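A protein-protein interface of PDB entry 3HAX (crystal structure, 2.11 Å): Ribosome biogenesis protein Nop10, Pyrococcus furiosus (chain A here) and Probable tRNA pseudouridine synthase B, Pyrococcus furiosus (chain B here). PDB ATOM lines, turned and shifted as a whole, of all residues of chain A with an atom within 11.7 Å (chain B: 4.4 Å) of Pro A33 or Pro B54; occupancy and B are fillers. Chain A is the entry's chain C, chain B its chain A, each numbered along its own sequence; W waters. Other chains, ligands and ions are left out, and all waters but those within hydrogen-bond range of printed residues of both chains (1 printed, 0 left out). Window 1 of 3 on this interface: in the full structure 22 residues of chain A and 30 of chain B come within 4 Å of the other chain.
Water W1 lies within hydrogen-bond range of the backbone carbonyl oxygen (O) of Ala A30 (2.7 Å) and the side-chain carboxylate (OD2) of Asp B52 (2.8 Å).
The backbone carbonyl oxygen (O) of Pro B57 is in hydrogen-bond range of the side-chain amino group (NZ) of Lys B53 (2.9 Å).
The side-chain amino group of Lys B53 is in hydrogen-bond range of the backbone carbonyl oxygen of Pro B83 (3.1 Å).
The side-chain carboxylate (OD2) of Asp A39 is in salt-bridge range of the guanidinium group (NH2) of Arg A45 (2.7 Å).
O of Val B85 lies within hydrogen-bond range of NZ of Lys B53 (2.8 Å).
Of chain B, only Pro B54 (3.7 Å) and His B218 (3.6 Å) come within 4 Å of Pro A33.
Of the printed residues of chain A, Pro B54 touches Pro A33 (3.7 Å).
Of chain A, only Pro A32 comes within 4 Å of Asp B52.
No residue of chain A comes within 4 Å of Gly B56.
No residue of chain A comes within 4 Å of Pro B57.
Printed residues of chain B within 4 Å of Lys A49: His B218 (3.8 Å).
Printed residues of chain A within 4 Å of His B218: Pro A33 (3.6 Å), Arg A34 (2.9 Å), Phe A35 (3.7 Å), Arg A45 (3.7 Å) and Lys A49 (3.8 Å).
Printed residues of chain B within 4 Å of His A31: Pro B55 (3.8 Å).
Of the printed residues of chain B, Phe A35 touches Leu B217 and His B218.
Of the printed residues of chain A, Leu B217 touches Phe A35.
His A31 touches Pro B55.
Pro A32 touches Asp B52.
O of Lys B53 touches CG of Pro A32 (3.5 Å).
Pro B55 touches Pro A32.
CB of Pro B54 touches O of Pro A33, at 3.7 Å.
Pro A33 touches His B218.
Phe A35 touches Leu B217.
Phe A35 touches His B218.
ND1 of His B218 touches NH1 of Arg A45 (3.7 Å).
O of His B218 touches NZ of Lys A49 (3.8 Å).
Of the 16 printed residues of chain A, 8 touch a printed residue of chain B.
Of the 10 printed residues of chain B, 6 touch a printed residue of chain A.
Hydrophobic or aromatic side chains of chain B that line the printed part of chain A: Pro B54, Pro B55, Leu B217 and His B218.
Among the printed residues, no Asp or Glu carboxylate lies within 4 Å of a Lys or Arg side-chain nitrogen of the other chain.
A ring nitrogen (NE2) of His B218 is in hydrogen-bond range of the backbone carbonyl oxygen (O) of Arg A34, at 2.9 Å.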
ATOM      1  N   PHE A   3     -12.145   2.064  12.200  1.00  0.00           N
ATOM      2  CA  PHE A   3     -13.010   1.129  11.423  1.00  0.00           C
ATOM      3  C   PHE A   3     -14.410   1.031  12.023  1.00  0.00           C
ATOM      4  O   PHE A   3     -14.574   1.071  13.245  1.00  0.00           O
ATOM      5  CB  PHE A   3     -12.369  -0.258  11.334  1.00  0.00           C
ATOM      6  CG  PHE A   3     -11.080  -0.283  10.561  1.00  0.00           C
ATOM      7  CD1 PHE A   3      -9.861  -0.401  11.222  1.00  0.00           C
ATOM      8  CD2 PHE A   3     -11.082  -0.188   9.170  1.00  0.00           C
ATOM      9  CE1 PHE A   3      -8.663  -0.426  10.510  1.00  0.00           C
ATOM     10  CE2 PHE A   3      -9.890  -0.214   8.451  1.00  0.00           C
ATOM     11  CZ  PHE A   3      -8.680  -0.332   9.122  1.00  0.00           C
ATOM     12  N   ILE A   5     -16.915  -1.363  10.609  1.00  0.00           N
ATOM     13  CA  ILE A   5     -17.465  -2.708  10.428  1.00  0.00           C
ATOM     14  C   ILE A   5     -17.099  -3.619  11.599  1.00  0.00           C
ATOM     15  O   ILE A   5     -15.922  -3.807  11.920  1.00  0.00           O
ATOM     16  CB  ILE A   5     -17.054  -3.351   9.073  1.00  0.00           C
ATOM     17  CG1 ILE A   5     -17.477  -2.456   7.898  1.00  0.00           C
ATOM     18  CG2 ILE A   5     -17.681  -4.738   8.933  1.00  0.00           C
ATOM     19  CD1 ILE A   5     -17.074  -2.974   6.519  1.00  0.00           C
ATOM     20  N   LYS A  28     -17.124  -7.482  17.825  1.00  0.00           N
ATOM     21  CA  LYS A  28     -15.713  -7.117  17.719  1.00  0.00           C
ATOM     22  C   LYS A  28     -15.421  -6.507  16.351  1.00  0.00           C
ATOM     23  O   LYS A  28     -16.137  -6.784  15.391  1.00  0.00           O
ATOM     24  CB  LYS A  28     -14.823  -8.343  17.956  1.00  0.00           C
ATOM     25  CG  LYS A  28     -14.876  -8.896  19.377  1.00  0.00           C
ATOM     26  CD  LYS A  28     -13.764  -9.903  19.616  1.00  0.00           C
ATOM     27  CE  LYS A  28     -13.695 -10.315  21.077  1.00  0.00           C
ATOM     28  NZ  LYS A  28     -12.495 -11.153  21.353  1.00  0.00           N
ATOM     29  N   VAL A  29     -14.379  -5.681  16.263  1.00  0.00           N
ATOM     30  CA  VAL A  29     -13.966  -5.088  14.984  1.00  0.00           C
ATOM     31  C   VAL A  29     -13.647  -6.207  13.984  1.00  0.00           C
ATOM     32  O   VAL A  29     -12.976  -7.182  14.328  1.00  0.00           O
ATOM     33  CB  VAL A  29     -12.750  -4.131  15.136  1.00  0.00           C
ATOM     34  CG1 VAL A  29     -12.455  -3.418  13.817  1.00  0.00           C
ATOM     35  CG2 VAL A  29     -12.999  -3.104  16.231  1.00  0.00           C
ATOM     36  N   ALA A  30     -14.148  -6.063  12.758  1.00  0.00           N
ATOM     37  CA  ALA A  30     -14.057  -7.118  11.743  1.00  0.00           C
ATOM     38  C   ALA A  30     -12.666  -7.282  11.133  1.00  0.00           C
ATOM     39  O   ALA A  30     -12.310  -8.367  10.666  1.00  0.00           O
ATOM     40  CB  ALA A  30     -15.087  -6.882  10.649  1.00  0.00           C
ATOM     41  N   HIS A  31     -11.886  -6.206  11.137  1.00  0.00           N
ATOM     42  CA  HIS A  31     -10.574  -6.189  10.487  1.00  0.00           C
ATOM     43  C   HIS A  31      -9.456  -6.656  11.419  1.00  0.00           C
ATOM     44  O   HIS A  31      -9.461  -6.319  12.601  1.00  0.00           O
ATOM     45  CB  HIS A  31     -10.268  -4.788   9.954  1.00  0.00           C
ATOM     46  CG  HIS A  31     -11.374  -4.208   9.130  1.00  0.00           C
ATOM     47  ND1 HIS A  31     -11.506  -4.456   7.780  1.00  0.00           N
ATOM     48  CD2 HIS A  31     -12.410  -3.405   9.468  1.00  0.00           C
ATOM     49  CE1 HIS A  31     -12.570  -3.825   7.321  1.00  0.00           C
ATOM     50  NE2 HIS A  31     -13.136  -3.178   8.325  1.00  0.00           N
ATOM     51  N   PRO A  32      -8.494  -7.436  10.884  1.00  0.00           N
ATOM     52  CA  PRO A  32      -7.367  -7.937  11.670  1.00  0.00           C
ATOM     53  C   PRO A  32      -6.382  -6.818  12.007  1.00  0.00           C
ATOM     54  O   PRO A  32      -6.309  -5.831  11.271  1.00  0.00           O
ATOM     55  CB  PRO A  32      -6.690  -8.950  10.731  1.00  0.00           C
ATOM     56  CG  PRO A  32      -7.582  -9.099   9.564  1.00  0.00           C
ATOM     57  CD  PRO A  32      -8.417  -7.879   9.482  1.00  0.00           C
ATOM     58  N   PRO A  33      -5.622  -6.970  13.110  1.00  0.00           N
ATOM     59  CA  PRO A  33      -4.645  -5.946  13.476  1.00  0.00           C
ATOM     60  C   PRO A  33      -3.472  -5.890  12.492  1.00  0.00           C
ATOM     61  O   PRO A  33      -3.239  -6.844  11.743  1.00  0.00           O
ATOM     62  CB  PRO A  33      -4.155  -6.406  14.852  1.00  0.00           C
ATOM     63  CG  PRO A  33      -4.359  -7.886  14.847  1.00  0.00           C
ATOM     64  CD  PRO A  33      -5.632  -8.090  14.071  1.00  0.00           C
ATOM     65  N   ARG A  34      -2.757  -4.769  12.504  1.00  0.00           N
ATOM     66  CA  ARG A  34      -1.551  -4.583  11.706  1.00  0.00           C
ATOM     67  C   ARG A  34      -0.530  -5.682  11.993  1.00  0.00           C
ATOM     68  O   ARG A  34      -0.266  -6.011  13.153  1.00  0.00           O
ATOM     69  CB  ARG A  34      -0.940  -3.206  11.998  1.00  0.00           C
ATOM     70  CG  ARG A  34       0.405  -2.931  11.315  1.00  0.00           C
ATOM     71  CD  ARG A  34       0.975  -1.562  11.688  1.00  0.00           C
ATOM     72  NE  ARG A  34       0.103  -0.466  11.264  1.00  0.00           N
ATOM     73  CZ  ARG A  34      -0.604   0.300  12.091  1.00  0.00           C
ATOM     74  NH1 ARG A  34      -0.545   0.110  13.406  1.00  0.00           N
ATOM     75  NH2 ARG A  34      -1.371   1.263  11.603  1.00  0.00           N
ATOM     76  N   PHE A  35       0.022  -6.251  10.927  1.00  0.00           N
ATOM     77  CA  PHE A  35       1.125  -7.198  11.041  1.00  0.00           C
ATOM     78  C   PHE A  35       2.381  -6.643  10.373  1.00  0.00           C
ATOM     79  O   PHE A  35       2.305  -5.923   9.372  1.00  0.00           O
ATOM     80  CB  PHE A  35       0.750  -8.561  10.443  1.00  0.00           C
ATOM     81  CG  PHE A  35       1.866  -9.574  10.493  1.00  0.00           C
ATOM     82  CD1 PHE A  35       2.129 -10.282  11.661  1.00  0.00           C
ATOM     83  CD2 PHE A  35       2.658  -9.814   9.372  1.00  0.00           C
ATOM     84  CE1 PHE A  35       3.163 -11.211  11.716  1.00  0.00           C
ATOM     85  CE2 PHE A  35       3.692 -10.744   9.413  1.00  0.00           C
ATOM     86  CZ  PHE A  35       3.946 -11.442  10.588  1.00  0.00           C
ATOM     87  N   SER A  36       3.531  -6.985  10.942  1.00  0.00           N
ATOM     88  CA  SER A  36       4.821  -6.650  10.359  1.00  0.00           C
ATOM     89  C   SER A  36       5.682  -7.905  10.235  1.00  0.00           C
ATOM     90  O   SER A  36       5.713  -8.720  11.158  1.00  0.00           O
ATOM     91  CB  SER A  36       5.540  -5.620  11.226  1.00  0.00           C
ATOM     92  OG  SER A  36       6.870  -5.436  10.776  1.00  0.00           O
ATOM     93  N   PRO A  37       6.384  -8.067   9.095  1.00  0.00           N
ATOM     94  CA  PRO A  37       7.342  -9.165   8.942  1.00  0.00           C
ATOM     95  C   PRO A  37       8.525  -9.051   9.911  1.00  0.00           C
ATOM     96  O   PRO A  37       9.156 -10.058  10.235  1.00  0.00           O
ATOM     97  CB  PRO A  37       7.816  -9.025   7.491  1.00  0.00           C
ATOM     98  CG  PRO A  37       7.516  -7.619   7.116  1.00  0.00           C
ATOM     99  CD  PRO A  37       6.297  -7.236   7.881  1.00  0.00           C
ATOM    100  N   ASP A  39       8.038  -7.980  12.978  1.00  0.00           N
ATOM    101  CA  ASP A  39       7.373  -8.481  14.189  1.00  0.00           C
ATOM    102  C   ASP A  39       8.214  -8.331  15.468  1.00  0.00           C
ATOM    103  O   ASP A  39       8.596  -9.331  16.078  1.00  0.00           O
ATOM    104  CB  ASP A  39       6.951  -9.944  13.978  1.00  0.00           C
ATOM    105  CG  ASP A  39       5.814 -10.373  14.895  1.00  0.00           C
ATOM    106  OD1 ASP A  39       5.060  -9.506  15.391  1.00  0.00           O
ATOM    107  OD2 ASP A  39       5.673 -11.596  15.108  1.00  0.00           O
ATOM    108  N   ARG A  45       4.188 -11.674  22.418  1.00  0.00           N
ATOM    109  CA  ARG A  45       2.861 -12.110  21.990  1.00  0.00           C
ATOM    110  C   ARG A  45       2.727 -13.634  22.069  1.00  0.00           C
ATOM    111  O   ARG A  45       1.684 -14.144  22.472  1.00  0.00           O
ATOM    112  CB  ARG A  45       2.550 -11.619  20.572  1.00  0.00           C
ATOM    113  CG  ARG A  45       1.130 -11.943  20.102  1.00  0.00           C
ATOM    114  CD  ARG A  45       0.891 -11.568  18.647  1.00  0.00           C
ATOM    115  NE  ARG A  45       1.722 -12.341  17.722  1.00  0.00           N
ATOM    116  CZ  ARG A  45       2.743 -11.838  17.035  1.00  0.00           C
ATOM    117  NH1 ARG A  45       3.064 -10.554  17.158  1.00  0.00           N
ATOM    118  NH2 ARG A  45       3.442 -12.614  16.219  1.00  0.00           N
ATOM    119  N   TRP A  48       2.271 -14.849  25.670  1.00  0.00           N
ATOM    120  CA  TRP A  48       0.867 -14.694  26.023  1.00  0.00           C
ATOM    121  C   TRP A  48       0.037 -15.818  25.402  1.00  0.00           C
ATOM    122  O   TRP A  48      -0.775 -16.444  26.084  1.00  0.00           O
ATOM    123  CB  TRP A  48       0.371 -13.317  25.568  1.00  0.00           C
ATOM    124  CG  TRP A  48      -1.112 -13.202  25.355  1.00  0.00           C
ATOM    125  CD1 TRP A  48      -2.084 -13.211  26.312  1.00  0.00           C
ATOM    126  CD2 TRP A  48      -1.786 -13.037  24.100  1.00  0.00           C
ATOM    127  NE1 TRP A  48      -3.322 -13.069  25.734  1.00  0.00           N
ATOM    128  CE2 TRP A  48      -3.169 -12.961  24.376  1.00  0.00           C
ATOM    129  CE3 TRP A  48      -1.355 -12.949  22.767  1.00  0.00           C
ATOM    130  CZ2 TRP A  48      -4.131 -12.802  23.369  1.00  0.00           C
ATOM    131  CZ3 TRP A  48      -2.313 -12.790  21.763  1.00  0.00           C
ATOM    132  CH2 TRP A  48      -3.683 -12.718  22.073  1.00  0.00           C
ATOM    133  N   LYS A  49       0.278 -16.082  24.119  1.00  0.00           N
ATOM    134  CA  LYS A  49      -0.488 -17.059  23.349  1.00  0.00           C
ATOM    135  C   LYS A  49      -0.315 -18.489  23.865  1.00  0.00           C
ATOM    136  O   LYS A  49      -1.287 -19.240  23.937  1.00  0.00           O
ATOM    137  CB  LYS A  49      -0.123 -16.963  21.866  1.00  0.00           C
ATOM    138  CG  LYS A  49      -1.142 -17.576  20.920  1.00  0.00           C
ATOM    139  CD  LYS A  49      -0.892 -17.149  19.474  1.00  0.00           C
ATOM    140  CE  LYS A  49      -1.428 -15.746  19.194  1.00  0.00           C
ATOM    141  NZ  LYS A  49      -1.281 -15.365  17.756  1.00  0.00           N
ATOM    142  N   ASP B  52      -6.686 -14.288   6.391  1.00  0.00           N
ATOM    143  CA  ASP B  52      -7.419 -13.071   6.693  1.00  0.00           C
ATOM    144  C   ASP B  52      -6.457 -11.897   6.541  1.00  0.00           C
ATOM    145  O   ASP B  52      -5.729 -11.551   7.474  1.00  0.00           O
ATOM    146  CB  ASP B  52      -7.995 -13.128   8.114  1.00  0.00           C
ATOM    147  CG  ASP B  52      -9.070 -12.071   8.365  1.00  0.00           C
ATOM    148  OD1 ASP B  52      -9.243 -11.159   7.524  1.00  0.00           O
ATOM    149  OD2 ASP B  52      -9.745 -12.150   9.415  1.00  0.00           O
ATOM    150  N   LYS B  53      -6.448 -11.304   5.348  1.00  0.00           N
ATOM    151  CA  LYS B  53      -5.577 -10.172   5.034  1.00  0.00           C
ATOM    152  C   LYS B  53      -5.863  -8.974   5.943  1.00  0.00           C
ATOM    153  O   LYS B  53      -7.021  -8.639   6.174  1.00  0.00           O
ATOM    154  CB  LYS B  53      -5.745  -9.770   3.564  1.00  0.00           C
ATOM    155  CG  LYS B  53      -4.854  -8.615   3.112  1.00  0.00           C
ATOM    156  CD  LYS B  53      -5.305  -8.063   1.769  1.00  0.00           C
ATOM    157  CE  LYS B  53      -4.563  -6.790   1.409  1.00  0.00           C
ATOM    158  NZ  LYS B  53      -4.841  -5.677   2.364  1.00  0.00           N
ATOM    159  N   PRO B  54      -4.803  -8.341   6.480  1.00  0.00           N
ATOM    160  CA  PRO B  54      -4.974  -7.101   7.234  1.00  0.00           C
ATOM    161  C   PRO B  54      -5.072  -5.876   6.320  1.00  0.00           C
ATOM    162  O   PRO B  54      -4.545  -5.899   5.203  1.00  0.00           O
ATOM    163  CB  PRO B  54      -3.692  -7.031   8.066  1.00  0.00           C
ATOM    164  CG  PRO B  54      -2.666  -7.701   7.217  1.00  0.00           C
ATOM    165  CD  PRO B  54      -3.391  -8.771   6.435  1.00  0.00           C
ATOM    166  N   PRO B  55      -5.751  -4.808   6.787  1.00  0.00           N
ATOM    167  CA  PRO B  55      -5.691  -3.544   6.061  1.00  0.00           C
ATOM    168  C   PRO B  55      -4.281  -2.972   6.169  1.00  0.00           C
ATOM    169  O   PRO B  55      -3.633  -3.122   7.211  1.00  0.00           O
ATOM    170  CB  PRO B  55      -6.677  -2.645   6.818  1.00  0.00           C
ATOM    171  CG  PRO B  55      -7.482  -3.563   7.680  1.00  0.00           C
ATOM    172  CD  PRO B  55      -6.587  -4.709   7.996  1.00  0.00           C
ATOM    173  N   GLY B  56      -3.816  -2.332   5.101  1.00  0.00           N
ATOM    174  CA  GLY B  56      -2.470  -1.771   5.057  1.00  0.00           C
ATOM    175  C   GLY B  56      -1.731  -2.157   3.789  1.00  0.00           C
ATOM    176  O   GLY B  56      -1.797  -1.435   2.795  1.00  0.00           O
ATOM    177  N   PRO B  57      -1.022  -3.303   3.815  1.00  0.00           N
ATOM    178  CA  PRO B  57      -0.246  -3.782   2.671  1.00  0.00           C
ATOM    179  C   PRO B  57      -1.108  -4.238   1.502  1.00  0.00           C
ATOM    180  O   PRO B  57      -2.266  -4.611   1.690  1.00  0.00           O
ATOM    181  CB  PRO B  57       0.496  -4.990   3.242  1.00  0.00           C
ATOM    182  CG  PRO B  57      -0.378  -5.473   4.352  1.00  0.00           C
ATOM    183  CD  PRO B  57      -0.918  -4.221   4.965  1.00  0.00           C
ATOM    184  N   PRO B  83      -5.062  -2.506  -0.823  1.00  0.00           N
ATOM    185  CA  PRO B  83      -4.338  -2.226   0.420  1.00  0.00           C
ATOM    186  C   PRO B  83      -5.230  -2.017   1.647  1.00  0.00           C
ATOM    187  O   PRO B  83      -4.983  -2.623   2.687  1.00  0.00           O
ATOM    188  CB  PRO B  83      -3.575  -0.939   0.091  1.00  0.00           C
ATOM    189  CG  PRO B  83      -3.339  -1.020  -1.363  1.00  0.00           C
ATOM    190  CD  PRO B  83      -4.545  -1.692  -1.942  1.00  0.00           C
ATOM    191  N   VAL B  85      -8.246  -2.971   2.077  1.00  0.00           N
ATOM    192  CA  VAL B  85      -9.259  -4.026   2.185  1.00  0.00           C
ATOM    193  C   VAL B  85      -8.740  -5.231   2.978  1.00  0.00           C
ATOM    194  O   VAL B  85      -7.590  -5.652   2.814  1.00  0.00           O
ATOM    195  CB  VAL B  85      -9.761  -4.459   0.778  1.00  0.00           C
ATOM    196  CG1 VAL B  85     -10.848  -5.527   0.868  1.00  0.00           C
ATOM    197  CG2 VAL B  85     -10.273  -3.244   0.007  1.00  0.00           C
ATOM    198  N   LEU B 217      -2.299 -13.229   9.853  1.00  0.00           N
ATOM    199  CA  LEU B 217      -0.846 -13.360   9.765  1.00  0.00           C
ATOM    200  C   LEU B 217      -0.213 -13.626  11.130  1.00  0.00           C
ATOM    201  O   LEU B 217       0.719 -14.421  11.229  1.00  0.00           O
ATOM    202  CB  LEU B 217      -0.230 -12.121   9.109  1.00  0.00           C
ATOM    203  CG  LEU B 217      -0.433 -11.991   7.594  1.00  0.00           C
ATOM    204  CD1 LEU B 217      -0.207 -10.558   7.140  1.00  0.00           C
ATOM    205  CD2 LEU B 217       0.478 -12.951   6.825  1.00  0.00           C
ATOM    206  N   HIS B 218      -0.737 -12.980  12.171  1.00  0.00           N
ATOM    207  CA  HIS B 218      -0.279 -13.200  13.546  1.00  0.00           C
ATOM    208  C   HIS B 218      -0.359 -14.665  13.965  1.00  0.00           C
ATOM    209  O   HIS B 218       0.631 -15.226  14.427  1.00  0.00           O
ATOM    210  CB  HIS B 218      -1.064 -12.336  14.533  1.00  0.00           C
ATOM    211  CG  HIS B 218      -0.884 -10.868  14.323  1.00  0.00           C
ATOM    212  ND1 HIS B 218       0.023 -10.119  15.040  1.00  0.00           N
ATOM    213  CD2 HIS B 218      -1.489 -10.010  13.468  1.00  0.00           C
ATOM    214  CE1 HIS B 218      -0.034  -8.861  14.640  1.00  0.00           C
ATOM    215  NE2 HIS B 218      -0.945  -8.768  13.689  1.00  0.00           N
HETATM  216  O   HOH W   1     -10.586 -10.268  11.342  1.00  0.00           O
